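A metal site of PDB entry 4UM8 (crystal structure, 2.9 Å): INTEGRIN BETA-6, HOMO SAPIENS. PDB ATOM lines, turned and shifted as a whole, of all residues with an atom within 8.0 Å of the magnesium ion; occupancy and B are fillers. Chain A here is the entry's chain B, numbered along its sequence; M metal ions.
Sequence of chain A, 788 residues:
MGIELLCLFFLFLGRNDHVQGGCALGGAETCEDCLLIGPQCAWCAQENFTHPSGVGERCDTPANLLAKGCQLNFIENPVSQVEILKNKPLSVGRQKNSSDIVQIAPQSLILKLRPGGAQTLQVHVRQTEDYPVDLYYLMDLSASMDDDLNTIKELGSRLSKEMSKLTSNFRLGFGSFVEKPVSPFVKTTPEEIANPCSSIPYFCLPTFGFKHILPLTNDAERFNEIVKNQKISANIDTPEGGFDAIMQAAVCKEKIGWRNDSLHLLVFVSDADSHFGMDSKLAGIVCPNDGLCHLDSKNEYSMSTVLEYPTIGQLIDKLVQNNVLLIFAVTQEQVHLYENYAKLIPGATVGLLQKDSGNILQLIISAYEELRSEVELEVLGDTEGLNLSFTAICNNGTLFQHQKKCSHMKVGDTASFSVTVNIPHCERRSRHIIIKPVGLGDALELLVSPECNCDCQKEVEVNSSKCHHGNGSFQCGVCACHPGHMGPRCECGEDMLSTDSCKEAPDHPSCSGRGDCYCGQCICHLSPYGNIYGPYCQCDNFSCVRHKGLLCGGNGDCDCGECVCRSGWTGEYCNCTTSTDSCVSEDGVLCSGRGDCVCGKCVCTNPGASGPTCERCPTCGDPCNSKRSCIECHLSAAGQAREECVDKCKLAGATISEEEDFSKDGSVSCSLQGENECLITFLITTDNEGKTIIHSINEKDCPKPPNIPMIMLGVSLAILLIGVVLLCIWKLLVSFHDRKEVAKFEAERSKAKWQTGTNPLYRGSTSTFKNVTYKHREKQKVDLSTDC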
ATOM      1  N   MET A 139     -30.050   6.393 -31.015  1.00  0.00           N
ATOM      2  CA  MET A 139     -28.789   5.928 -30.438  1.00  0.00           C
ATOM      3  C   MET A 139     -27.615   6.888 -30.615  1.00  0.00           C
ATOM      4  O   MET A 139     -27.451   7.515 -31.667  1.00  0.00           O
ATOM      5  CB  MET A 139     -28.400   4.567 -31.022  1.00  0.00           C
ATOM      6  CG  MET A 139     -27.129   3.990 -30.424  1.00  0.00           C
ATOM      7  SD  MET A 139     -26.672   2.390 -31.100  1.00  0.00           S
ATOM      8  CE  MET A 139     -26.695   2.770 -32.856  1.00  0.00           C
ATOM      9  N   ASP A 140     -26.800   7.003 -29.571  1.00  0.00           N
ATOM     10  CA  ASP A 140     -25.540   7.721 -29.625  1.00  0.00           C
ATOM     11  C   ASP A 140     -24.534   6.956 -30.477  1.00  0.00           C
ATOM     12  O   ASP A 140     -24.327   5.758 -30.265  1.00  0.00           O
ATOM     13  CB  ASP A 140     -24.996   7.931 -28.204  1.00  0.00           C
ATOM     14  CG  ASP A 140     -23.759   8.811 -28.170  1.00  0.00           C
ATOM     15  OD1 ASP A 140     -23.225   9.175 -29.241  1.00  0.00           O
ATOM     16  OD2 ASP A 140     -23.296   9.130 -27.055  1.00  0.00           O
ATOM     17  N   LEU A 141     -23.907   7.639 -31.427  1.00  0.00           N
ATOM     18  CA  LEU A 141     -22.916   6.992 -32.280  1.00  0.00           C
ATOM     19  C   LEU A 141     -21.496   7.476 -31.991  1.00  0.00           C
ATOM     20  O   LEU A 141     -20.662   7.533 -32.893  1.00  0.00           O
ATOM     21  CB  LEU A 141     -23.241   7.231 -33.760  1.00  0.00           C
ATOM     22  CG  LEU A 141     -24.291   6.315 -34.381  1.00  0.00           C
ATOM     23  CD1 LEU A 141     -24.382   6.552 -35.881  1.00  0.00           C
ATOM     24  CD2 LEU A 141     -23.954   4.868 -34.091  1.00  0.00           C
ATOM     25  N   SER A 142     -21.231   7.826 -30.732  1.00  0.00           N
ATOM     26  CA  SER A 142     -19.882   8.160 -30.331  1.00  0.00           C
ATOM     27  C   SER A 142     -19.012   6.909 -30.404  1.00  0.00           C
ATOM     28  O   SER A 142     -19.524   5.792 -30.347  1.00  0.00           O
ATOM     29  CB  SER A 142     -19.848   8.751 -28.917  1.00  0.00           C
ATOM     30  OG  SER A 142     -20.631   7.983 -28.014  1.00  0.00           O
ATOM     31  N   ALA A 143     -17.712   7.096 -30.552  1.00  0.00           N
ATOM     32  CA  ALA A 143     -16.779   5.975 -30.732  1.00  0.00           C
ATOM     33  C   ALA A 143     -16.822   4.995 -29.553  1.00  0.00           C
ATOM     34  O   ALA A 143     -16.451   3.831 -29.689  1.00  0.00           O
ATOM     35  CB  ALA A 143     -15.376   6.485 -30.936  1.00  0.00           C
ATOM     36  N   SER A 144     -17.286   5.469 -28.398  1.00  0.00           N
ATOM     37  CA  SER A 144     -17.395   4.632 -27.217  1.00  0.00           C
ATOM     38  C   SER A 144     -18.625   3.728 -27.285  1.00  0.00           C
ATOM     39  O   SER A 144     -18.861   2.919 -26.387  1.00  0.00           O
ATOM     40  CB  SER A 144     -17.448   5.495 -25.954  1.00  0.00           C
ATOM     41  OG  SER A 144     -18.501   6.433 -26.020  1.00  0.00           O
ATOM     42  N   MET A 145     -19.408   3.885 -28.344  1.00  0.00           N
ATOM     43  CA  MET A 145     -20.588   3.048 -28.569  1.00  0.00           C
ATOM     44  C   MET A 145     -20.321   2.028 -29.666  1.00  0.00           C
ATOM     45  O   MET A 145     -21.245   1.450 -30.228  1.00  0.00           O
ATOM     46  CB  MET A 145     -21.798   3.913 -28.918  1.00  0.00           C
ATOM     47  CG  MET A 145     -22.151   4.949 -27.861  1.00  0.00           C
ATOM     48  SD  MET A 145     -22.815   4.214 -26.357  1.00  0.00           S
ATOM     49  CE  MET A 145     -24.469   3.770 -26.900  1.00  0.00           C
ATOM     50  N   PHE A 177     -27.456  10.280 -33.301  1.00  0.00           N
ATOM     51  CA  PHE A 177     -27.002  11.621 -32.924  1.00  0.00           C
ATOM     52  C   PHE A 177     -25.568  11.598 -32.391  1.00  0.00           C
ATOM     53  O   PHE A 177     -25.077  10.551 -31.968  1.00  0.00           O
ATOM     54  CB  PHE A 177     -27.925  12.212 -31.854  1.00  0.00           C
ATOM     55  CG  PHE A 177     -27.831  11.536 -30.520  1.00  0.00           C
ATOM     56  CD1 PHE A 177     -26.915  11.975 -29.565  1.00  0.00           C
ATOM     57  CD2 PHE A 177     -28.641  10.461 -30.214  1.00  0.00           C
ATOM     58  CE1 PHE A 177     -26.816  11.345 -28.337  1.00  0.00           C
ATOM     59  CE2 PHE A 177     -28.552   9.827 -28.976  1.00  0.00           C
ATOM     60  CZ  PHE A 177     -27.645  10.274 -28.046  1.00  0.00           C
ATOM     61  N   VAL A 178     -24.910  12.751 -32.421  1.00  0.00           N
ATOM     62  CA  VAL A 178     -23.625  12.924 -31.747  1.00  0.00           C
ATOM     63  C   VAL A 178     -23.567  14.287 -31.049  1.00  0.00           C
ATOM     64  O   VAL A 178     -23.754  14.382 -29.837  1.00  0.00           O
ATOM     65  CB  VAL A 178     -22.419  12.801 -32.712  1.00  0.00           C
ATOM     66  CG1 VAL A 178     -21.114  12.975 -31.950  1.00  0.00           C
ATOM     67  CG2 VAL A 178     -22.423  11.468 -33.429  1.00  0.00           C
ATOM     68  N   ALA A 234     -17.125  10.668 -33.733  1.00  0.00           N
ATOM     69  CA  ALA A 234     -16.058  11.119 -32.847  1.00  0.00           C
ATOM     70  C   ALA A 234     -16.120  10.435 -31.488  1.00  0.00           C
ATOM     71  O   ALA A 234     -17.178   9.998 -31.051  1.00  0.00           O
ATOM     72  CB  ALA A 234     -16.105  12.626 -32.681  1.00  0.00           C
ATOM     73  N   ASN A 235     -14.969  10.340 -30.830  1.00  0.00           N
ATOM     74  CA  ASN A 235     -14.914   9.900 -29.441  1.00  0.00           C
ATOM     75  C   ASN A 235     -14.999  11.108 -28.518  1.00  0.00           C
ATOM     76  O   ASN A 235     -14.077  11.930 -28.452  1.00  0.00           O
ATOM     77  CB  ASN A 235     -13.649   9.088 -29.159  1.00  0.00           C
ATOM     78  CG  ASN A 235     -12.385   9.785 -29.628  1.00  0.00           C
ATOM     79  OD1 ASN A 235     -12.417  10.586 -30.552  1.00  0.00           O
ATOM     80  ND2 ASN A 235     -11.269   9.479 -28.973  1.00  0.00           N
ATOM     81  N   ILE A 236     -16.103  11.222 -27.795  1.00  0.00           N
ATOM     82  CA  ILE A 236     -16.370  12.398 -26.970  1.00  0.00           C
ATOM     83  C   ILE A 236     -16.596  12.042 -25.508  1.00  0.00           C
ATOM     84  O   ILE A 236     -17.504  11.277 -25.176  1.00  0.00           O
ATOM     85  CB  ILE A 236     -17.588  13.171 -27.506  1.00  0.00           C
ATOM     86  CG1 ILE A 236     -17.443  13.436 -29.001  1.00  0.00           C
ATOM     87  CG2 ILE A 236     -17.749  14.476 -26.760  1.00  0.00           C
ATOM     88  CD1 ILE A 236     -18.545  14.302 -29.583  1.00  0.00           C
ATOM     89  N   ASP A 237     -15.759  12.589 -24.627  1.00  0.00           N
ATOM     90  CA  ASP A 237     -15.914  12.389 -23.194  1.00  0.00           C
ATOM     91  C   ASP A 237     -16.717  13.508 -22.547  1.00  0.00           C
ATOM     92  O   ASP A 237     -16.939  13.510 -21.337  1.00  0.00           O
ATOM     93  CB  ASP A 237     -14.543  12.283 -22.513  1.00  0.00           C
ATOM     94  CG  ASP A 237     -13.428  11.962 -23.495  1.00  0.00           C
ATOM     95  OD1 ASP A 237     -13.529  12.364 -24.672  1.00  0.00           O
ATOM     96  OD2 ASP A 237     -12.452  11.306 -23.087  1.00  0.00           O
ATOM     97  N   THR A 238     -17.152  14.467 -23.356  1.00  0.00           N
ATOM     98  CA  THR A 238     -17.967  15.572 -22.877  1.00  0.00           C
ATOM     99  C   THR A 238     -19.427  15.259 -23.188  1.00  0.00           C
ATOM    100  O   THR A 238     -19.714  14.381 -24.005  1.00  0.00           O
ATOM    101  CB  THR A 238     -17.542  16.915 -23.515  1.00  0.00           C
ATOM    102  OG1 THR A 238     -17.897  16.929 -24.909  1.00  0.00           O
ATOM    103  CG2 THR A 238     -16.047  17.134 -23.362  1.00  0.00           C
ATOM    104  N   PRO A 239     -20.370  15.959 -22.518  1.00  0.00           N
ATOM    105  CA  PRO A 239     -21.787  15.804 -22.864  1.00  0.00           C
ATOM    106  C   PRO A 239     -22.067  15.994 -24.354  1.00  0.00           C
ATOM    107  O   PRO A 239     -21.339  16.720 -25.034  1.00  0.00           O
ATOM    108  CB  PRO A 239     -22.487  16.899 -22.034  1.00  0.00           C
ATOM    109  CG  PRO A 239     -21.373  17.729 -21.452  1.00  0.00           C
ATOM    110  CD  PRO A 239     -20.197  16.823 -21.351  1.00  0.00           C
ATOM    111  N   GLU A 240     -23.097  15.329 -24.849  1.00  0.00           N
ATOM    112  CA  GLU A 240     -23.365  15.291 -26.287  1.00  0.00           C
ATOM    113  C   GLU A 240     -24.708  15.917 -26.649  1.00  0.00           C
ATOM    114  O   GLU A 240     -25.544  16.151 -25.782  1.00  0.00           O
ATOM    115  CB  GLU A 240     -23.301  13.843 -26.782  1.00  0.00           C
ATOM    116  CG  GLU A 240     -21.971  13.154 -26.468  1.00  0.00           C
ATOM    117  CD  GLU A 240     -21.879  11.783 -27.115  1.00  0.00           C
ATOM    118  OE1 GLU A 240     -22.487  11.606 -28.189  1.00  0.00           O
ATOM    119  OE2 GLU A 240     -21.196  10.893 -26.562  1.00  0.00           O
ATOM    120  N   VAL A 269     -30.497   6.120 -26.188  1.00  0.00           N
ATOM    121  CA  VAL A 269     -29.380   5.251 -25.845  1.00  0.00           C
ATOM    122  C   VAL A 269     -28.050   5.978 -25.931  1.00  0.00           C
ATOM    123  O   VAL A 269     -27.525   6.203 -27.030  1.00  0.00           O
ATOM    124  CB  VAL A 269     -29.334   4.011 -26.756  1.00  0.00           C
ATOM    125  CG1 VAL A 269     -28.203   3.088 -26.333  1.00  0.00           C
ATOM    126  CG2 VAL A 269     -30.654   3.268 -26.727  1.00  0.00           C
ATOM    127  N   SER A 270     -27.485   6.322 -24.784  1.00  0.00           N
ATOM    128  CA  SER A 270     -26.222   7.044 -24.734  1.00  0.00           C
ATOM    129  C   SER A 270     -25.362   6.610 -23.545  1.00  0.00           C
ATOM    130  O   SER A 270     -25.825   5.895 -22.661  1.00  0.00           O
ATOM    131  CB  SER A 270     -26.471   8.554 -24.679  1.00  0.00           C
ATOM    132  OG  SER A 270     -25.258   9.282 -24.671  1.00  0.00           O
ATOM    133  N   ASP A 271     -24.112   7.065 -23.541  1.00  0.00           N
ATOM    134  CA  ASP A 271     -23.187   6.715 -22.468  1.00  0.00           C
ATOM    135  C   ASP A 271     -22.525   7.966 -21.892  1.00  0.00           C
ATOM    136  O   ASP A 271     -21.426   7.905 -21.337  1.00  0.00           O
ATOM    137  CB  ASP A 271     -22.123   5.739 -22.968  1.00  0.00           C
ATOM    138  CG  ASP A 271     -21.273   6.318 -24.081  1.00  0.00           C
ATOM    139  OD1 ASP A 271     -21.755   7.200 -24.826  1.00  0.00           O
ATOM    140  OD2 ASP A 271     -20.105   5.886 -24.213  1.00  0.00           O
ATOM    141  N   ALA A 272     -23.204   9.101 -22.037  1.00  0.00           N
ATOM    142  CA  ALA A 272     -22.669  10.364 -21.551  1.00  0.00           C
ATOM    143  C   ALA A 272     -23.796  11.349 -21.254  1.00  0.00           C
ATOM    144  O   ALA A 272     -24.971  11.073 -21.512  1.00  0.00           O
ATOM    145  CB  ALA A 272     -21.695  10.967 -22.552  1.00  0.00           C
ATOM    146  N   ASP A 273     -23.422  12.509 -20.717  1.00  0.00           N
ATOM    147  CA  ASP A 273     -24.390  13.546 -20.384  1.00  0.00           C
ATOM    148  C   ASP A 273     -24.844  14.243 -21.674  1.00  0.00           C
ATOM    149  O   ASP A 273     -24.386  13.897 -22.759  1.00  0.00           O
ATOM    150  CB  ASP A 273     -23.777  14.545 -19.382  1.00  0.00           C
ATOM    151  CG  ASP A 273     -24.785  15.565 -18.873  1.00  0.00           C
ATOM    152  OD1 ASP A 273     -25.844  15.164 -18.351  1.00  0.00           O
ATOM    153  OD2 ASP A 273     -24.501  16.775 -18.976  1.00  0.00           O
HETATM  154 MG    MG M   1     -21.390   8.799 -26.238  1.00  0.00          MG
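The side-chain hydroxyl (OG) of Ser 144 is in hydrogen-bond range of the side-chain carboxylate (OD2) of Asp 271, 2.5 Å away.
N of Glu 240 is in hydrogen-bond range of O of Asp 273 (2.8 Å).
O of Val 269 sits at hydrogen-bond distance from N of Asp 140 (2.8 Å).
The side-chain carboxylate (OD2) of Asp 140 sits close to the side-chain hydroxyl (OG) of Ser 270.
The side-chain hydroxyl of Ser 144 sits close to the side-chain hydroxyl of Ser 142 (3.3 Å).
Ser 144 touches the magnesium ion (OG to MG, 3.7 Å).
The nearest printed residue that does not touch the magnesium ion is Ser 270 (4.2 Å).
The magnesium ion is bound by OG of Ser 142 (2.1 Å), OD2 of Asp 140 (2.1 Å), OE2 of Glu 240 (2.1 Å) and OD1 of Asp 271 (2.2 Å).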
